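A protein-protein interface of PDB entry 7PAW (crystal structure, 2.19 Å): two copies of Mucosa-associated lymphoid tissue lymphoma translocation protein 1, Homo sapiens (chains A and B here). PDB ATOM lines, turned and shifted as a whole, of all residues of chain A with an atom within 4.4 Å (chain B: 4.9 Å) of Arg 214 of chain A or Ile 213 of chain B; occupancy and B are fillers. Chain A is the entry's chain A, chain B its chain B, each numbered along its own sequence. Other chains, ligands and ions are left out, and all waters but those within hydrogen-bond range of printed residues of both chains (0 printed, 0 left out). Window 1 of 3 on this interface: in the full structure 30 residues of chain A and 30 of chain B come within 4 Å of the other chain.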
ATOM      1  N   ARG A 128       4.052 -13.867  38.975  1.00  0.00           N
ATOM      2  CA  ARG A 128       4.163 -15.317  38.886  1.00  0.00           C
ATOM      3  C   ARG A 128       5.331 -15.907  39.628  1.00  0.00           C
ATOM      4  O   ARG A 128       5.816 -16.972  39.255  1.00  0.00           O
ATOM      5  CB  ARG A 128       4.190 -15.743  37.423  1.00  0.00           C
ATOM      6  CG  ARG A 128       2.932 -15.415  36.681  1.00  0.00           C
ATOM      7  CD  ARG A 128       3.097 -15.757  35.245  1.00  0.00           C
ATOM      8  NE  ARG A 128       3.175 -17.206  35.035  1.00  0.00           N
ATOM      9  CZ  ARG A 128       3.639 -17.763  33.926  1.00  0.00           C
ATOM     10  NH1 ARG A 128       4.064 -17.007  32.925  1.00  0.00           N
ATOM     11  NH2 ARG A 128       3.682 -19.081  33.809  1.00  0.00           N
ATOM     12  N   ILE A 149      -8.417 -24.498  25.677  1.00  0.00           N
ATOM     13  CA  ILE A 149      -7.879 -23.774  26.834  1.00  0.00           C
ATOM     14  C   ILE A 149      -6.836 -22.757  26.392  1.00  0.00           C
ATOM     15  O   ILE A 149      -5.836 -23.121  25.774  1.00  0.00           O
ATOM     16  CB  ILE A 149      -7.265 -24.759  27.903  1.00  0.00           C
ATOM     17  CG1 ILE A 149      -8.251 -25.868  28.324  1.00  0.00           C
ATOM     18  CG2 ILE A 149      -6.751 -23.980  29.127  1.00  0.00           C
ATOM     19  CD1 ILE A 149      -7.602 -27.169  28.806  1.00  0.00           C
ATOM     20  N   VAL A 150      -7.049 -21.487  26.739  1.00  0.00           N
ATOM     21  CA  VAL A 150      -6.094 -20.415  26.429  1.00  0.00           C
ATOM     22  C   VAL A 150      -5.755 -19.624  27.660  1.00  0.00           C
ATOM     23  O   VAL A 150      -6.650 -19.079  28.289  1.00  0.00           O
ATOM     24  CB  VAL A 150      -6.535 -19.498  25.251  1.00  0.00           C
ATOM     25  CG1 VAL A 150      -5.499 -18.401  24.996  1.00  0.00           C
ATOM     26  CG2 VAL A 150      -6.786 -20.304  23.972  1.00  0.00           C
ATOM     27  N   PHE A 151      -4.452 -19.571  28.021  1.00  0.00           N
ATOM     28  CA  PHE A 151      -3.935 -18.742  29.133  1.00  0.00           C
ATOM     29  C   PHE A 151      -3.177 -17.576  28.554  1.00  0.00           C
ATOM     30  O   PHE A 151      -2.334 -17.741  27.661  1.00  0.00           O
ATOM     31  CB  PHE A 151      -2.997 -19.493  30.084  1.00  0.00           C
ATOM     32  CG  PHE A 151      -3.682 -20.384  31.082  1.00  0.00           C
ATOM     33  CD1 PHE A 151      -4.096 -21.666  30.727  1.00  0.00           C
ATOM     34  CD2 PHE A 151      -3.875 -19.963  32.392  1.00  0.00           C
ATOM     35  CE1 PHE A 151      -4.734 -22.494  31.663  1.00  0.00           C
ATOM     36  CE2 PHE A 151      -4.551 -20.775  33.315  1.00  0.00           C
ATOM     37  CZ  PHE A 151      -4.969 -22.035  32.950  1.00  0.00           C
ATOM     38  N   TYR A 153      -0.929 -14.836  30.211  1.00  0.00           N
ATOM     39  CA  TYR A 153      -0.281 -14.339  31.426  1.00  0.00           C
ATOM     40  C   TYR A 153       0.347 -13.016  31.130  1.00  0.00           C
ATOM     41  O   TYR A 153       1.060 -12.915  30.137  1.00  0.00           O
ATOM     42  CB  TYR A 153       0.803 -15.274  31.932  1.00  0.00           C
ATOM     43  CG  TYR A 153       0.356 -16.681  32.255  1.00  0.00           C
ATOM     44  CD1 TYR A 153       0.475 -17.699  31.318  1.00  0.00           C
ATOM     45  CD2 TYR A 153      -0.030 -17.029  33.548  1.00  0.00           C
ATOM     46  CE1 TYR A 153       0.201 -19.019  31.646  1.00  0.00           C
ATOM     47  CE2 TYR A 153      -0.349 -18.342  33.877  1.00  0.00           C
ATOM     48  CZ  TYR A 153      -0.224 -19.337  32.922  1.00  0.00           C
ATOM     49  OH  TYR A 153      -0.544 -20.633  33.228  1.00  0.00           O
ATOM     50  N   GLN A 157       7.075 -16.745  33.808  1.00  0.00           N
ATOM     51  CA  GLN A 157       7.279 -17.489  35.055  1.00  0.00           C
ATOM     52  C   GLN A 157       8.458 -16.964  35.845  1.00  0.00           C
ATOM     53  O   GLN A 157       9.536 -16.767  35.278  1.00  0.00           O
ATOM     54  CB  GLN A 157       7.522 -18.954  34.718  1.00  0.00           C
ATOM     55  CG  GLN A 157       6.741 -19.944  35.553  1.00  0.00           C
ATOM     56  CD  GLN A 157       6.617 -21.269  34.836  1.00  0.00           C
ATOM     57  OE1 GLN A 157       7.437 -21.629  33.975  1.00  0.00           O
ATOM     58  NE2 GLN A 157       5.581 -22.030  35.172  1.00  0.00           N
ATOM     59  N   GLU A 212       3.081 -14.247  28.439  1.00  0.00           N
ATOM     60  CA  GLU A 212       3.241 -15.664  28.195  1.00  0.00           C
ATOM     61  C   GLU A 212       1.902 -16.275  27.800  1.00  0.00           C
ATOM     62  O   GLU A 212       0.907 -16.083  28.500  1.00  0.00           O
ATOM     63  CB  GLU A 212       3.902 -16.429  29.329  1.00  0.00           C
ATOM     64  CG  GLU A 212       4.457 -17.747  28.804  1.00  0.00           C
ATOM     65  CD  GLU A 212       4.426 -18.952  29.719  1.00  0.00           C
ATOM     66  OE1 GLU A 212       4.425 -20.084  29.192  1.00  0.00           O
ATOM     67  OE2 GLU A 212       4.426 -18.775  30.955  1.00  0.00           O
ATOM     68  N   ILE A 213       1.880 -16.975  26.656  1.00  0.00           N
ATOM     69  CA  ILE A 213       0.678 -17.612  26.136  1.00  0.00           C
ATOM     70  C   ILE A 213       0.783 -19.109  26.202  1.00  0.00           C
ATOM     71  O   ILE A 213       1.700 -19.675  25.625  1.00  0.00           O
ATOM     72  CB  ILE A 213       0.324 -17.137  24.691  1.00  0.00           C
ATOM     73  CG1 ILE A 213       0.033 -15.635  24.663  1.00  0.00           C
ATOM     74  CG2 ILE A 213      -0.884 -17.918  24.113  1.00  0.00           C
ATOM     75  CD1 ILE A 213       0.619 -15.001  23.518  1.00  0.00           C
ATOM     76  N   ARG A 214      -0.157 -19.742  26.902  1.00  0.00           N
ATOM     77  CA  ARG A 214      -0.276 -21.189  26.931  1.00  0.00           C
ATOM     78  C   ARG A 214      -1.589 -21.534  26.196  1.00  0.00           C
ATOM     79  O   ARG A 214      -2.617 -20.914  26.433  1.00  0.00           O
ATOM     80  CB  ARG A 214      -0.241 -21.737  28.352  1.00  0.00           C
ATOM     81  CG  ARG A 214       1.106 -21.547  28.967  1.00  0.00           C
ATOM     82  CD  ARG A 214       1.237 -22.136  30.346  1.00  0.00           C
ATOM     83  NE  ARG A 214       2.599 -21.899  30.809  1.00  0.00           N
ATOM     84  CZ  ARG A 214       3.079 -22.262  31.988  1.00  0.00           C
ATOM     85  NH1 ARG A 214       2.289 -22.840  32.885  1.00  0.00           N
ATOM     86  NH2 ARG A 214       4.354 -22.037  32.287  1.00  0.00           N
ATOM     87  N   SER A 215      -1.543 -22.451  25.258  1.00  0.00           N
ATOM     88  CA  SER A 215      -2.753 -22.751  24.510  1.00  0.00           C
ATOM     89  C   SER A 215      -2.862 -24.171  24.022  1.00  0.00           C
ATOM     90  O   SER A 215      -1.910 -24.682  23.469  1.00  0.00           O
ATOM     91  CB  SER A 215      -2.912 -21.785  23.340  1.00  0.00           C
ATOM     92  OG  SER A 215      -4.037 -22.155  22.565  1.00  0.00           O
ATOM     93  N   VAL B 150       9.790 -20.828  22.705  1.00  0.00           N
ATOM     94  CA  VAL B 150       8.580 -21.464  22.186  1.00  0.00           C
ATOM     95  C   VAL B 150       8.605 -22.973  22.507  1.00  0.00           C
ATOM     96  O   VAL B 150       9.530 -23.687  22.132  1.00  0.00           O
ATOM     97  CB  VAL B 150       8.335 -21.152  20.675  1.00  0.00           C
ATOM     98  CG1 VAL B 150       7.019 -21.754  20.195  1.00  0.00           C
ATOM     99  CG2 VAL B 150       8.359 -19.636  20.412  1.00  0.00           C
ATOM    100  N   PHE B 151       7.604 -23.434  23.244  1.00  0.00           N
ATOM    101  CA  PHE B 151       7.419 -24.846  23.575  1.00  0.00           C
ATOM    102  C   PHE B 151       6.242 -25.416  22.792  1.00  0.00           C
ATOM    103  O   PHE B 151       5.147 -24.843  22.801  1.00  0.00           O
ATOM    104  CB  PHE B 151       7.155 -25.050  25.067  1.00  0.00           C
ATOM    105  CG  PHE B 151       8.371 -25.242  25.927  1.00  0.00           C
ATOM    106  CD1 PHE B 151       9.075 -24.151  26.413  1.00  0.00           C
ATOM    107  CD2 PHE B 151       8.800 -26.516  26.278  1.00  0.00           C
ATOM    108  CE1 PHE B 151      10.237 -24.331  27.181  1.00  0.00           C
ATOM    109  CE2 PHE B 151       9.929 -26.694  27.087  1.00  0.00           C
ATOM    110  CZ  PHE B 151      10.653 -25.601  27.518  1.00  0.00           C
ATOM    111  N   GLY B 152       6.476 -26.548  22.144  1.00  0.00           N
ATOM    112  CA  GLY B 152       5.450 -27.280  21.419  1.00  0.00           C
ATOM    113  C   GLY B 152       5.382 -28.684  21.964  1.00  0.00           C
ATOM    114  O   GLY B 152       6.265 -29.490  21.685  1.00  0.00           O
ATOM    115  N   LEU B 192       2.713 -23.341  14.765  1.00  0.00           N
ATOM    116  CA  LEU B 192       2.352 -24.375  15.734  1.00  0.00           C
ATOM    117  C   LEU B 192       0.836 -24.408  16.044  1.00  0.00           C
ATOM    118  O   LEU B 192       0.268 -25.489  16.170  1.00  0.00           O
ATOM    119  CB  LEU B 192       3.201 -24.250  17.018  1.00  0.00           C
ATOM    120  CG  LEU B 192       4.655 -24.739  16.925  1.00  0.00           C
ATOM    121  CD1 LEU B 192       5.343 -24.655  18.283  1.00  0.00           C
ATOM    122  CD2 LEU B 192       4.742 -26.168  16.372  1.00  0.00           C
ATOM    123  N   ASP B 193       0.190 -23.226  16.079  1.00  0.00           N
ATOM    124  CA  ASP B 193      -1.242 -23.003  16.319  1.00  0.00           C
ATOM    125  C   ASP B 193      -2.109 -23.611  15.205  1.00  0.00           C
ATOM    126  O   ASP B 193      -3.178 -24.167  15.471  1.00  0.00           O
ATOM    127  CB  ASP B 193      -1.476 -21.479  16.437  1.00  0.00           C
ATOM    128  CG  ASP B 193      -2.917 -21.005  16.464  1.00  0.00           C
ATOM    129  OD1 ASP B 193      -3.568 -21.159  17.517  1.00  0.00           O
ATOM    130  OD2 ASP B 193      -3.380 -20.435  15.434  1.00  0.00           O
ATOM    131  N   ALA B 196      -2.098 -27.342  15.506  1.00  0.00           N
ATOM    132  CA  ALA B 196      -3.028 -27.647  16.603  1.00  0.00           C
ATOM    133  C   ALA B 196      -4.428 -27.742  16.038  1.00  0.00           C
ATOM    134  O   ALA B 196      -5.160 -28.665  16.394  1.00  0.00           O
ATOM    135  CB  ALA B 196      -2.961 -26.572  17.678  1.00  0.00           C
ATOM    136  N   LEU B 211      -2.187 -30.802  20.825  1.00  0.00           N
ATOM    137  CA  LEU B 211      -0.936 -30.072  20.936  1.00  0.00           C
ATOM    138  C   LEU B 211      -1.094 -28.940  21.973  1.00  0.00           C
ATOM    139  O   LEU B 211      -2.146 -28.310  22.026  1.00  0.00           O
ATOM    140  CB  LEU B 211      -0.668 -29.442  19.562  1.00  0.00           C
ATOM    141  CG  LEU B 211       0.759 -29.348  19.066  1.00  0.00           C
ATOM    142  CD1 LEU B 211       0.766 -29.101  17.602  1.00  0.00           C
ATOM    143  CD2 LEU B 211       1.489 -28.204  19.698  1.00  0.00           C
ATOM    144  N   GLU B 212      -0.068 -28.713  22.811  1.00  0.00           N
ATOM    145  CA  GLU B 212      -0.055 -27.588  23.748  1.00  0.00           C
ATOM    146  C   GLU B 212       1.133 -26.704  23.437  1.00  0.00           C
ATOM    147  O   GLU B 212       2.264 -27.186  23.386  1.00  0.00           O
ATOM    148  CB  GLU B 212      -0.042 -28.002  25.213  1.00  0.00           C
ATOM    149  CG  GLU B 212      -0.292 -26.809  26.114  1.00  0.00           C
ATOM    150  CD  GLU B 212       0.062 -26.940  27.574  1.00  0.00           C
ATOM    151  OE1 GLU B 212      -0.079 -28.047  28.138  1.00  0.00           O
ATOM    152  OE2 GLU B 212       0.456 -25.914  28.167  1.00  0.00           O
ATOM    153  N   ILE B 213       0.864 -25.406  23.207  1.00  0.00           N
ATOM    154  CA  ILE B 213       1.875 -24.407  22.890  1.00  0.00           C
ATOM    155  C   ILE B 213       2.049 -23.498  24.081  1.00  0.00           C
ATOM    156  O   ILE B 213       1.052 -23.077  24.642  1.00  0.00           O
ATOM    157  CB  ILE B 213       1.512 -23.626  21.578  1.00  0.00           C
ATOM    158  CG1 ILE B 213       1.251 -24.565  20.388  1.00  0.00           C
ATOM    159  CG2 ILE B 213       2.575 -22.574  21.199  1.00  0.00           C
ATOM    160  CD1 ILE B 213       0.013 -24.157  19.611  1.00  0.00           C
ATOM    161  N   ARG B 214       3.309 -23.247  24.506  1.00  0.00           N
ATOM    162  CA  ARG B 214       3.694 -22.300  25.575  1.00  0.00           C
ATOM    163  C   ARG B 214       4.704 -21.364  24.937  1.00  0.00           C
ATOM    164  O   ARG B 214       5.751 -21.811  24.469  1.00  0.00           O
ATOM    165  CB  ARG B 214       4.304 -22.990  26.803  1.00  0.00           C
ATOM    166  CG  ARG B 214       3.319 -23.873  27.520  1.00  0.00           C
ATOM    167  CD  ARG B 214       3.855 -24.433  28.798  1.00  0.00           C
ATOM    168  NE  ARG B 214       2.833 -25.234  29.465  1.00  0.00           N
ATOM    169  CZ  ARG B 214       3.034 -25.968  30.558  1.00  0.00           C
ATOM    170  NH1 ARG B 214       4.240 -26.027  31.117  1.00  0.00           N
ATOM    171  NH2 ARG B 214       2.034 -26.663  31.091  1.00  0.00           N
ATOM    172  N   SER B 215       4.367 -20.083  24.832  1.00  0.00           N
ATOM    173  CA  SER B 215       5.266 -19.139  24.174  1.00  0.00           C
ATOM    174  C   SER B 215       5.446 -17.820  24.903  1.00  0.00           C
ATOM    175  O   SER B 215       4.511 -17.309  25.502  1.00  0.00           O
ATOM    176  CB  SER B 215       4.801 -18.892  22.746  1.00  0.00           C
ATOM    177  OG  SER B 215       5.455 -17.782  22.159  1.00  0.00           O
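Arg 214 of chain A touches just these residues of chain B: Ile 213 (3.3 Å) and Arg 214 (3.5 Å). Of chain A, only Ile 213, Arg 214 and Ser 215 come within 4 Å of Ile 213 of chain B. Printed residues of chain A within 4 Å of Arg 214 of chain B: Glu 212, Ile 213 and Arg 214. Of the printed residues of chain B, Glu 212 of chain A touches Arg 214 (3.8 Å) and Ser 215 (3.3 Å). Printed residues of chain A within 4 Å of Glu 212 of chain B: Ser 215. Printed residues of chain B within 4 Å of Ser 215 of chain A: Leu 211, Glu 212 and Ile 213. The nearest residue of chain B that does not touch Arg 214 of chain A is Glu 212 of chain B (4.2 Å). The nearest printed residue of chain A that does not touch Ile 213 of chain B is Glu 212 of chain A (6.4 Å). The nearest printed residue of chain A that does not touch Leu 211 of chain B is Ile 149 of chain A (7.4 Å).
Among the printed residues, merely in contact across the chains: Glu 212 of chain A with Arg 214 of chain B (3.8 Å), Glu 212 of chain A with Ser 215 of chain B (3.3 Å), Ile 213 of chain A with Ile 213 of chain B (3.6 Å), Ile 213 of chain A with Arg 214 of chain B (3.3 Å), Arg 214 of chain A with Ile 213 of chain B (3.3 Å), Arg 214 of chain A with Arg 214 of chain B (3.5 Å), Ser 215 of chain A with Leu 211 of chain B (3.9 Å) and Ser 215 of chain A with Glu 212 of chain B (3.5 Å).
The guanidinium group (NH2) of Arg 214 of chain A lies close to the side-chain amide nitrogen (NE2) of Gln 157 of chain A (3.1 Å). The guanidinium group (NE) of Arg 214 of chain A lies within salt-bridge range of the side-chain carboxylate (OE1) of Glu 212 of chain A (3.0 Å). OE2 of Glu 212 of chain B is in salt-bridge range of NE of Arg 214 of chain B (2.8 Å). The backbone carbonyl oxygen of Glu 212 of chain A lies within hydrogen-bond range of the backbone NH of Tyr 153 of chain A, at 2.8 Å. NH1 of Arg 128 of chain A is in salt-bridge range of OE2 of Glu 212 of chain A (2.7 Å). The backbone NH (N) of Phe 151 of chain A sits at hydrogen-bond distance from the backbone carbonyl oxygen (O) of Arg 214 of chain A, 2.8 Å away.
The backbone NH (N) of Ser 215 of chain A sits at hydrogen-bond distance from the backbone carbonyl oxygen (O) of Ile 213 of chain B, at 2.7 Å. The backbone NH (N) of Ser 215 of chain B lies within hydrogen-bond range of the backbone carbonyl oxygen (O) of Ile 213 of chain A (2.8 Å).
Glu 212 of chain A touches Ser 215 of chain B, and with the chains exchanged Ser 215 of chain A touches Glu 212 of chain B. Ile 213 of chain B touches its own counterpart, Ile 213 of chain A. Ile 213 of chain A touches Arg 214 of chain B, and with the chains exchanged Arg 214 of chain A touches Ile 213 of chain B. Ile 213 of chain A touches Ser 215 of chain B, and with the chains exchanged Ser 215 of chain A touches Ile 213 of chain B. Of the 10 pairs that touch across the chains among the printed residues, 8 have their exchanged pair printed and touching as well.
Among the printed residues, no Asp or Glu carboxylate lies within 4 Å of a Lys or Arg side-chain nitrogen of the other chain.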
